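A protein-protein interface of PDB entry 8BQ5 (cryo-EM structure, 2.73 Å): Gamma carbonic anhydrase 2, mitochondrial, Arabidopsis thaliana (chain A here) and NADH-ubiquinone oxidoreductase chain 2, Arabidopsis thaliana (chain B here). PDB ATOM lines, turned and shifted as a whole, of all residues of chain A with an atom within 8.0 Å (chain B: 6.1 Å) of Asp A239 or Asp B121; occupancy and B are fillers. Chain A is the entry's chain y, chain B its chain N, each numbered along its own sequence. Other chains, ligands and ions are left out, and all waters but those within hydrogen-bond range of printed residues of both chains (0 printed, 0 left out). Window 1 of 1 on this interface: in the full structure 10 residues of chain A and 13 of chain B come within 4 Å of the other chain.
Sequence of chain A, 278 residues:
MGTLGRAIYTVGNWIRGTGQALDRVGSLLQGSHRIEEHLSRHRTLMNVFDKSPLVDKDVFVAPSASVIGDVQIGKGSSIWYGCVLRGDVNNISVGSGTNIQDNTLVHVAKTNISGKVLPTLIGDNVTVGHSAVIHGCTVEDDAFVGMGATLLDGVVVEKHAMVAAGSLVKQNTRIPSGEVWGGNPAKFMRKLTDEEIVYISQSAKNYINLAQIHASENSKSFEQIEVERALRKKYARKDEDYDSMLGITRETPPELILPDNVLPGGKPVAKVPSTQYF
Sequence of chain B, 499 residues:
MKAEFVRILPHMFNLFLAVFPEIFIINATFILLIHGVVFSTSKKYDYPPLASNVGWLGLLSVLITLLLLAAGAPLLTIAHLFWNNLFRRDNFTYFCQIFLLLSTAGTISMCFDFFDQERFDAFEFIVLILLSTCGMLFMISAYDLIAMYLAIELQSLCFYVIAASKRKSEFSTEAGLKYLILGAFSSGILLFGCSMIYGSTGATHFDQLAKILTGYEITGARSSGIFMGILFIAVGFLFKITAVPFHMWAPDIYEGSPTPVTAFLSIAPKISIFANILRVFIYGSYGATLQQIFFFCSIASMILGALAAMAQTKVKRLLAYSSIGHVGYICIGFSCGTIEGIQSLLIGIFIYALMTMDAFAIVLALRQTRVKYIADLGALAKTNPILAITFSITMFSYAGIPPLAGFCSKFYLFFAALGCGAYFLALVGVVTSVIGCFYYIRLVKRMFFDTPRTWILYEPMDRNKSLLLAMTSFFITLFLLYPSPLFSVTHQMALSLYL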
ATOM      1  N   ARG A 237      -2.336 -24.187 -29.807  1.00  0.00           N
ATOM      2  CA  ARG A 237      -3.223 -23.802 -28.721  1.00  0.00           C
ATOM      3  C   ARG A 237      -3.380 -24.989 -27.777  1.00  0.00           C
ATOM      4  O   ARG A 237      -2.761 -26.040 -27.965  1.00  0.00           O
ATOM      5  CB  ARG A 237      -4.572 -23.326 -29.267  1.00  0.00           C
ATOM      6  CG  ARG A 237      -4.454 -22.259 -30.336  1.00  0.00           C
ATOM      7  CD  ARG A 237      -4.309 -20.885 -29.715  1.00  0.00           C
ATOM      8  NE  ARG A 237      -4.943 -19.859 -30.531  1.00  0.00           N
ATOM      9  CZ  ARG A 237      -4.290 -19.039 -31.344  1.00  0.00           C
ATOM     10  NH1 ARG A 237      -2.971 -19.071 -31.444  1.00  0.00           N
ATOM     11  NH2 ARG A 237      -4.978 -18.167 -32.074  1.00  0.00           N
ATOM     12  N   LYS A 238      -4.210 -24.823 -26.749  1.00  0.00           N
ATOM     13  CA  LYS A 238      -4.399 -25.883 -25.767  1.00  0.00           C
ATOM     14  C   LYS A 238      -5.794 -25.795 -25.164  1.00  0.00           C
ATOM     15  O   LYS A 238      -6.455 -24.757 -25.220  1.00  0.00           O
ATOM     16  CB  LYS A 238      -3.334 -25.822 -24.665  1.00  0.00           C
ATOM     17  CG  LYS A 238      -2.816 -24.425 -24.385  1.00  0.00           C
ATOM     18  CD  LYS A 238      -1.674 -24.457 -23.384  1.00  0.00           C
ATOM     19  CE  LYS A 238      -0.498 -25.258 -23.910  1.00  0.00           C
ATOM     20  NZ  LYS A 238       0.689 -25.128 -23.023  1.00  0.00           N
ATOM     21  N   ASP A 239      -6.244 -26.930 -24.610  1.00  0.00           N
ATOM     22  CA  ASP A 239      -7.505 -27.045 -23.863  1.00  0.00           C
ATOM     23  C   ASP A 239      -7.251 -27.908 -22.627  1.00  0.00           C
ATOM     24  O   ASP A 239      -7.919 -28.924 -22.428  1.00  0.00           O
ATOM     25  CB  ASP A 239      -8.615 -27.610 -24.721  1.00  0.00           C
ATOM     26  CG  ASP A 239      -9.976 -27.529 -24.045  1.00  0.00           C
ATOM     27  OD1 ASP A 239     -10.061 -26.973 -22.930  1.00  0.00           O
ATOM     28  OD2 ASP A 239     -10.964 -28.008 -24.636  1.00  0.00           O
ATOM     29  N   GLU A 240      -6.243 -27.530 -21.834  1.00  0.00           N
ATOM     30  CA  GLU A 240      -5.843 -28.314 -20.666  1.00  0.00           C
ATOM     31  C   GLU A 240      -7.025 -28.725 -19.786  1.00  0.00           C
ATOM     32  O   GLU A 240      -6.940 -29.737 -19.084  1.00  0.00           O
ATOM     33  CB  GLU A 240      -4.823 -27.525 -19.848  1.00  0.00           C
ATOM     34  CG  GLU A 240      -3.755 -26.849 -20.694  1.00  0.00           C
ATOM     35  CD  GLU A 240      -3.464 -25.429 -20.250  1.00  0.00           C
ATOM     36  OE1 GLU A 240      -2.310 -25.154 -19.862  1.00  0.00           O
ATOM     37  OE2 GLU A 240      -4.387 -24.587 -20.295  1.00  0.00           O
ATOM     38  N   ASP A 241      -8.122 -27.964 -19.802  1.00  0.00           N
ATOM     39  CA  ASP A 241      -9.299 -28.335 -19.020  1.00  0.00           C
ATOM     40  C   ASP A 241      -9.931 -29.630 -19.526  1.00  0.00           C
ATOM     41  O   ASP A 241     -10.250 -30.531 -18.737  1.00  0.00           O
ATOM     42  CB  ASP A 241     -10.315 -27.196 -19.055  1.00  0.00           C
ATOM     43  CG  ASP A 241     -11.324 -27.283 -17.941  1.00  0.00           C
ATOM     44  OD1 ASP A 241     -12.434 -26.739 -18.107  1.00  0.00           O
ATOM     45  OD2 ASP A 241     -11.008 -27.894 -16.900  1.00  0.00           O
ATOM     46  N   TYR A 242     -10.119 -29.742 -20.840  1.00  0.00           N
ATOM     47  CA  TYR A 242     -10.655 -30.977 -21.396  1.00  0.00           C
ATOM     48  C   TYR A 242      -9.653 -32.117 -21.288  1.00  0.00           C
ATOM     49  O   TYR A 242     -10.051 -33.281 -21.174  1.00  0.00           O
ATOM     50  CB  TYR A 242     -11.070 -30.759 -22.846  1.00  0.00           C
ATOM     51  CG  TYR A 242     -12.090 -31.755 -23.332  1.00  0.00           C
ATOM     52  CD1 TYR A 242     -13.422 -31.642 -22.965  1.00  0.00           C
ATOM     53  CD2 TYR A 242     -11.723 -32.801 -24.163  1.00  0.00           C
ATOM     54  CE1 TYR A 242     -14.357 -32.548 -23.405  1.00  0.00           C
ATOM     55  CE2 TYR A 242     -12.652 -33.711 -24.611  1.00  0.00           C
ATOM     56  CZ  TYR A 242     -13.971 -33.578 -24.231  1.00  0.00           C
ATOM     57  OH  TYR A 242     -14.904 -34.482 -24.672  1.00  0.00           O
ATOM     58  N   ASP A 243      -8.356 -31.808 -21.328  1.00  0.00           N
ATOM     59  CA  ASP A 243      -7.352 -32.835 -21.081  1.00  0.00           C
ATOM     60  C   ASP A 243      -7.481 -33.389 -19.670  1.00  0.00           C
ATOM     61  O   ASP A 243      -7.414 -34.605 -19.462  1.00  0.00           O
ATOM     62  CB  ASP A 243      -5.951 -32.269 -21.308  1.00  0.00           C
ATOM     63  CG  ASP A 243      -5.645 -32.040 -22.772  1.00  0.00           C
ATOM     64  OD1 ASP A 243      -5.649 -33.024 -23.536  1.00  0.00           O
ATOM     65  OD2 ASP A 243      -5.388 -30.882 -23.159  1.00  0.00           O
ATOM     66  N   SER A 244      -7.677 -32.508 -18.687  1.00  0.00           N
ATOM     67  CA  SER A 244      -7.848 -32.960 -17.312  1.00  0.00           C
ATOM     68  C   SER A 244      -9.132 -33.762 -17.154  1.00  0.00           C
ATOM     69  O   SER A 244      -9.182 -34.716 -16.370  1.00  0.00           O
ATOM     70  CB  SER A 244      -7.832 -31.766 -16.359  1.00  0.00           C
ATOM     71  OG  SER A 244      -9.131 -31.237 -16.180  1.00  0.00           O
ATOM     72  N   MET A 245     -10.187 -33.387 -17.883  1.00  0.00           N
ATOM     73  CA  MET A 245     -11.388 -34.217 -17.877  1.00  0.00           C
ATOM     74  C   MET A 245     -11.103 -35.595 -18.464  1.00  0.00           C
ATOM     75  O   MET A 245     -11.614 -36.608 -17.973  1.00  0.00           O
ATOM     76  CB  MET A 245     -12.526 -33.543 -18.643  1.00  0.00           C
ATOM     77  CG  MET A 245     -13.848 -34.298 -18.519  1.00  0.00           C
ATOM     78  SD  MET A 245     -15.001 -34.041 -19.876  1.00  0.00           S
ATOM     79  CE  MET A 245     -14.318 -35.157 -21.093  1.00  0.00           C
ATOM     80  N   LEU A 246     -10.289 -35.652 -19.521  1.00  0.00           N
ATOM     81  CA  LEU A 246      -9.919 -36.920 -20.138  1.00  0.00           C
ATOM     82  C   LEU A 246      -8.837 -37.663 -19.367  1.00  0.00           C
ATOM     83  O   LEU A 246      -8.587 -38.834 -19.664  1.00  0.00           O
ATOM     84  CB  LEU A 246      -9.435 -36.689 -21.569  1.00  0.00           C
ATOM     85  CG  LEU A 246     -10.483 -36.518 -22.667  1.00  0.00           C
ATOM     86  CD1 LEU A 246      -9.861 -35.806 -23.846  1.00  0.00           C
ATOM     87  CD2 LEU A 246     -11.040 -37.861 -23.094  1.00  0.00           C
ATOM     88  N   ILE A 248      -5.491 -36.915 -19.325  1.00  0.00           N
ATOM     89  CA  ILE A 248      -4.287 -37.006 -20.138  1.00  0.00           C
ATOM     90  C   ILE A 248      -3.517 -35.697 -20.032  1.00  0.00           C
ATOM     91  O   ILE A 248      -4.063 -34.651 -19.676  1.00  0.00           O
ATOM     92  CB  ILE A 248      -4.596 -37.321 -21.617  1.00  0.00           C
ATOM     93  CG1 ILE A 248      -5.338 -36.151 -22.264  1.00  0.00           C
ATOM     94  CG2 ILE A 248      -5.399 -38.600 -21.740  1.00  0.00           C
ATOM     95  CD1 ILE A 248      -5.291 -36.165 -23.769  1.00  0.00           C
ATOM     96  N   ARG A 250      -0.876 -33.484 -22.451  1.00  0.00           N
ATOM     97  CA  ARG A 250      -0.271 -33.336 -23.765  1.00  0.00           C
ATOM     98  C   ARG A 250       1.078 -32.643 -23.646  1.00  0.00           C
ATOM     99  O   ARG A 250       1.181 -31.550 -23.083  1.00  0.00           O
ATOM    100  CB  ARG A 250      -1.196 -32.552 -24.691  1.00  0.00           C
ATOM    101  CG  ARG A 250      -2.586 -33.150 -24.785  1.00  0.00           C
ATOM    102  CD  ARG A 250      -3.294 -32.714 -26.046  1.00  0.00           C
ATOM    103  NE  ARG A 250      -4.684 -33.152 -26.064  1.00  0.00           N
ATOM    104  CZ  ARG A 250      -5.120 -34.219 -26.719  1.00  0.00           C
ATOM    105  NH1 ARG A 250      -4.301 -34.977 -27.429  1.00  0.00           N
ATOM    106  NH2 ARG A 250      -6.410 -34.534 -26.659  1.00  0.00           N
ATOM    107  N   PRO B  48      -8.237 -37.289 -30.019  1.00  0.00           N
ATOM    108  CA  PRO B  48      -8.405 -36.114 -30.860  1.00  0.00           C
ATOM    109  C   PRO B  48      -9.566 -35.259 -30.393  1.00  0.00           C
ATOM    110  O   PRO B  48     -10.596 -35.780 -29.941  1.00  0.00           O
ATOM    111  CB  PRO B  48      -8.678 -36.718 -32.242  1.00  0.00           C
ATOM    112  CG  PRO B  48      -9.382 -37.994 -31.942  1.00  0.00           C
ATOM    113  CD  PRO B  48      -8.865 -38.483 -30.610  1.00  0.00           C
ATOM    114  N   PRO B  49      -9.429 -33.939 -30.464  1.00  0.00           N
ATOM    115  CA  PRO B  49     -10.597 -33.071 -30.293  1.00  0.00           C
ATOM    116  C   PRO B  49     -11.615 -33.353 -31.385  1.00  0.00           C
ATOM    117  O   PRO B  49     -11.268 -33.491 -32.559  1.00  0.00           O
ATOM    118  CB  PRO B  49     -10.011 -31.659 -30.411  1.00  0.00           C
ATOM    119  CG  PRO B  49      -8.552 -31.826 -30.144  1.00  0.00           C
ATOM    120  CD  PRO B  49      -8.200 -33.167 -30.699  1.00  0.00           C
ATOM    121  N   LEU B  50     -12.884 -33.439 -30.994  1.00  0.00           N
ATOM    122  CA  LEU B  50     -13.941 -33.779 -31.937  1.00  0.00           C
ATOM    123  C   LEU B  50     -15.062 -32.754 -31.965  1.00  0.00           C
ATOM    124  O   LEU B  50     -16.133 -33.046 -32.505  1.00  0.00           O
ATOM    125  CB  LEU B  50     -14.520 -35.160 -31.622  1.00  0.00           C
ATOM    126  CG  LEU B  50     -13.579 -36.359 -31.709  1.00  0.00           C
ATOM    127  CD1 LEU B  50     -14.349 -37.632 -31.420  1.00  0.00           C
ATOM    128  CD2 LEU B  50     -12.912 -36.423 -33.068  1.00  0.00           C
ATOM    129  N   ALA B  51     -14.850 -31.565 -31.399  1.00  0.00           N
ATOM    130  CA  ALA B  51     -15.909 -30.564 -31.394  1.00  0.00           C
ATOM    131  C   ALA B  51     -16.277 -30.146 -32.811  1.00  0.00           C
ATOM    132  O   ALA B  51     -17.460 -30.000 -33.131  1.00  0.00           O
ATOM    133  CB  ALA B  51     -15.491 -29.353 -30.563  1.00  0.00           C
ATOM    134  N   PHE B 115     -14.187 -23.349 -31.793  1.00  0.00           N
ATOM    135  CA  PHE B 115     -13.686 -24.671 -31.423  1.00  0.00           C
ATOM    136  C   PHE B 115     -12.192 -24.796 -31.697  1.00  0.00           C
ATOM    137  O   PHE B 115     -11.434 -25.278 -30.850  1.00  0.00           O
ATOM    138  CB  PHE B 115     -14.459 -25.756 -32.172  1.00  0.00           C
ATOM    139  CG  PHE B 115     -15.879 -25.896 -31.729  1.00  0.00           C
ATOM    140  CD1 PHE B 115     -16.296 -25.364 -30.522  1.00  0.00           C
ATOM    141  CD2 PHE B 115     -16.806 -26.531 -32.533  1.00  0.00           C
ATOM    142  CE1 PHE B 115     -17.607 -25.487 -30.114  1.00  0.00           C
ATOM    143  CE2 PHE B 115     -18.118 -26.653 -32.133  1.00  0.00           C
ATOM    144  CZ  PHE B 115     -18.519 -26.130 -30.921  1.00  0.00           C
ATOM    145  N   GLU B 118      -9.781 -21.197 -29.931  1.00  0.00           N
ATOM    146  CA  GLU B 118      -9.867 -21.248 -28.477  1.00  0.00           C
ATOM    147  C   GLU B 118      -9.411 -22.600 -27.954  1.00  0.00           C
ATOM    148  O   GLU B 118      -8.920 -22.699 -26.824  1.00  0.00           O
ATOM    149  CB  GLU B 118     -11.301 -20.959 -28.028  1.00  0.00           C
ATOM    150  CG  GLU B 118     -11.493 -20.820 -26.531  1.00  0.00           C
ATOM    151  CD  GLU B 118     -11.289 -19.401 -26.047  1.00  0.00           C
ATOM    152  OE1 GLU B 118     -11.972 -18.489 -26.563  1.00  0.00           O
ATOM    153  OE2 GLU B 118     -10.447 -19.194 -25.150  1.00  0.00           O
ATOM    154  N   ARG B 119      -9.524 -23.634 -28.784  1.00  0.00           N
ATOM    155  CA  ARG B 119      -9.487 -25.031 -28.362  1.00  0.00           C
ATOM    156  C   ARG B 119     -10.487 -25.267 -27.230  1.00  0.00           C
ATOM    157  O   ARG B 119     -10.155 -25.400 -26.057  1.00  0.00           O
ATOM    158  CB  ARG B 119      -8.076 -25.499 -28.008  1.00  0.00           C
ATOM    159  CG  ARG B 119      -7.180 -25.519 -29.226  1.00  0.00           C
ATOM    160  CD  ARG B 119      -7.107 -26.892 -29.887  1.00  0.00           C
ATOM    161  NE  ARG B 119      -7.179 -28.001 -28.945  1.00  0.00           N
ATOM    162  CZ  ARG B 119      -6.154 -28.440 -28.229  1.00  0.00           C
ATOM    163  NH1 ARG B 119      -4.967 -27.862 -28.295  1.00  0.00           N
ATOM    164  NH2 ARG B 119      -6.322 -29.490 -27.431  1.00  0.00           N
ATOM    165  N   PHE B 120     -11.747 -25.186 -27.635  1.00  0.00           N
ATOM    166  CA  PHE B 120     -12.858 -25.815 -26.932  1.00  0.00           C
ATOM    167  C   PHE B 120     -13.065 -27.178 -27.585  1.00  0.00           C
ATOM    168  O   PHE B 120     -13.665 -27.276 -28.656  1.00  0.00           O
ATOM    169  CB  PHE B 120     -14.098 -24.936 -27.027  1.00  0.00           C
ATOM    170  CG  PHE B 120     -15.221 -25.354 -26.133  1.00  0.00           C
ATOM    171  CD1 PHE B 120     -16.083 -26.366 -26.517  1.00  0.00           C
ATOM    172  CD2 PHE B 120     -15.437 -24.714 -24.927  1.00  0.00           C
ATOM    173  CE1 PHE B 120     -17.129 -26.745 -25.705  1.00  0.00           C
ATOM    174  CE2 PHE B 120     -16.482 -25.088 -24.111  1.00  0.00           C
ATOM    175  CZ  PHE B 120     -17.329 -26.106 -24.500  1.00  0.00           C
ATOM    176  N   ASP B 121     -12.555 -28.238 -26.956  1.00  0.00           N
ATOM    177  CA  ASP B 121     -12.584 -29.562 -27.569  1.00  0.00           C
ATOM    178  C   ASP B 121     -13.800 -30.398 -27.188  1.00  0.00           C
ATOM    179  O   ASP B 121     -13.906 -31.539 -27.644  1.00  0.00           O
ATOM    180  CB  ASP B 121     -11.319 -30.363 -27.226  1.00  0.00           C
ATOM    181  CG  ASP B 121     -10.040 -29.619 -27.545  1.00  0.00           C
ATOM    182  OD1 ASP B 121      -9.960 -28.972 -28.608  1.00  0.00           O
ATOM    183  OD2 ASP B 121      -9.086 -29.738 -26.756  1.00  0.00           O
ATOM    184  N   ALA B 122     -14.719 -29.874 -26.382  1.00  0.00           N
ATOM    185  CA  ALA B 122     -15.842 -30.675 -25.896  1.00  0.00           C
ATOM    186  C   ALA B 122     -16.876 -30.859 -26.999  1.00  0.00           C
ATOM    187  O   ALA B 122     -17.548 -29.902 -27.396  1.00  0.00           O
ATOM    188  CB  ALA B 122     -16.470 -30.016 -24.672  1.00  0.00           C
ATOM    189  N   PHE B 123     -17.022 -32.093 -27.491  1.00  0.00           N
ATOM    190  CA  PHE B 123     -18.083 -32.376 -28.451  1.00  0.00           C
ATOM    191  C   PHE B 123     -19.456 -32.413 -27.793  1.00  0.00           C
ATOM    192  O   PHE B 123     -20.464 -32.267 -28.490  1.00  0.00           O
ATOM    193  CB  PHE B 123     -17.828 -33.702 -29.169  1.00  0.00           C
ATOM    194  CG  PHE B 123     -18.057 -34.907 -28.308  1.00  0.00           C
ATOM    195  CD1 PHE B 123     -17.047 -35.396 -27.505  1.00  0.00           C
ATOM    196  CD2 PHE B 123     -19.289 -35.543 -28.292  1.00  0.00           C
ATOM    197  CE1 PHE B 123     -17.257 -36.500 -26.709  1.00  0.00           C
ATOM    198  CE2 PHE B 123     -19.503 -36.643 -27.495  1.00  0.00           C
ATOM    199  CZ  PHE B 123     -18.486 -37.122 -26.701  1.00  0.00           C
ATOM    200  N   GLU B 124     -19.519 -32.620 -26.476  1.00  0.00           N
ATOM    201  CA  GLU B 124     -20.804 -32.681 -25.787  1.00  0.00           C
ATOM    202  C   GLU B 124     -21.555 -31.360 -25.857  1.00  0.00           C
ATOM    203  O   GLU B 124     -22.772 -31.337 -25.651  1.00  0.00           O
ATOM    204  CB  GLU B 124     -20.601 -33.097 -24.331  1.00  0.00           C
ATOM    205  CG  GLU B 124     -20.046 -34.502 -24.165  1.00  0.00           C
ATOM    206  CD  GLU B 124     -18.537 -34.531 -24.049  1.00  0.00           C
ATOM    207  OE1 GLU B 124     -17.877 -33.617 -24.583  1.00  0.00           O
ATOM    208  OE2 GLU B 124     -18.010 -35.474 -23.424  1.00  0.00           O
ATOM    209  N   LYS B 166     -17.439 -23.495 -19.809  1.00  0.00           N
ATOM    210  CA  LYS B 166     -16.071 -23.132 -19.439  1.00  0.00           C
ATOM    211  C   LYS B 166     -15.967 -23.286 -17.929  1.00  0.00           C
ATOM    212  O   LYS B 166     -16.005 -22.313 -17.177  1.00  0.00           O
ATOM    213  CB  LYS B 166     -15.731 -21.715 -19.884  1.00  0.00           C
ATOM    214  CG  LYS B 166     -15.761 -21.504 -21.384  1.00  0.00           C
ATOM    215  CD  LYS B 166     -14.419 -21.018 -21.906  1.00  0.00           C
ATOM    216  CE  LYS B 166     -13.358 -22.099 -21.763  1.00  0.00           C
ATOM    217  NZ  LYS B 166     -12.047 -21.701 -22.346  1.00  0.00           N
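The guanidinium group (NH1) of Arg B119 sits at hydrogen-bond distance from the backbone carbonyl oxygen (O) of Arg A237 (2.9 Å).
The backbone NH (N) of Asp B121 sits at hydrogen-bond distance from the side-chain carboxylate (OD2) of Asp A239, at 2.8 Å.
The side-chain carboxylate (OE1) of Glu B124 is in hydrogen-bond range of the side-chain hydroxyl (OH) of Tyr A242, at 3.1 Å.
N of Lys A238 sits close to NH1 of Arg B119 (3.5 Å).
The backbone carbonyl oxygen (O) of Arg B119 sits close to the side-chain carboxylate (OD2) of Asp A239, 3.1 Å away.
Hydrophobic or aromatic side chains of chain B within 4 Å of the printed part of chain A: Ala B122 and Phe B123.
Hydrophobic or aromatic side chains of chain A within 4 Å of the printed part of chain B: Tyr A242.
Among the printed residues, 10 pairs touch across the chains.
Among the printed residues, no Asp or Glu carboxylate lies within 4 Å of a Lys or Arg side-chain nitrogen of the other chain.
O of Phe B115 is in hydrogen-bond range of N of Phe B120, 3.2 Å away.
The side-chain carboxylate (OD2) of Asp B121 is in salt-bridge range of the guanidinium group (NH2) of Arg B119, at 2.9 Å.
The side-chain carboxylate (OD1) of Asp A239 sits at hydrogen-bond distance from the backbone NH (N) of Tyr A242.
Asp A239 touches three residues of chain B.
Of chain A, only Asp A239 and Tyr A242 come within 4 Å of Asp B121.
Ala B122 touches just one residue of chain A: Tyr A242 (3.5 Å).
Of the printed residues of chain A, Arg B119 touches Arg A237 (2.9 Å), Lys A238 (3.3 Å) and Asp A239 (2.9 Å).
Of the printed residues of chain B, Lys A238 touches Glu B118 (3.6 Å) and Arg B119 (3.3 Å).
Printed residues of chain A within 4 Å of Phe B123: Tyr A242.
Printed residues of chain A within 4 Å of Phe B120: Asp A239.
Phe B115 touches none of the printed residues of chain A.
Among the printed residues, merely in contact across the chains: Tyr A242 with Ala B122, Lys A238 with Glu B118, Tyr A242 with Phe B123, Asp A239 with Phe B120 and Tyr A242 with Asp B121.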
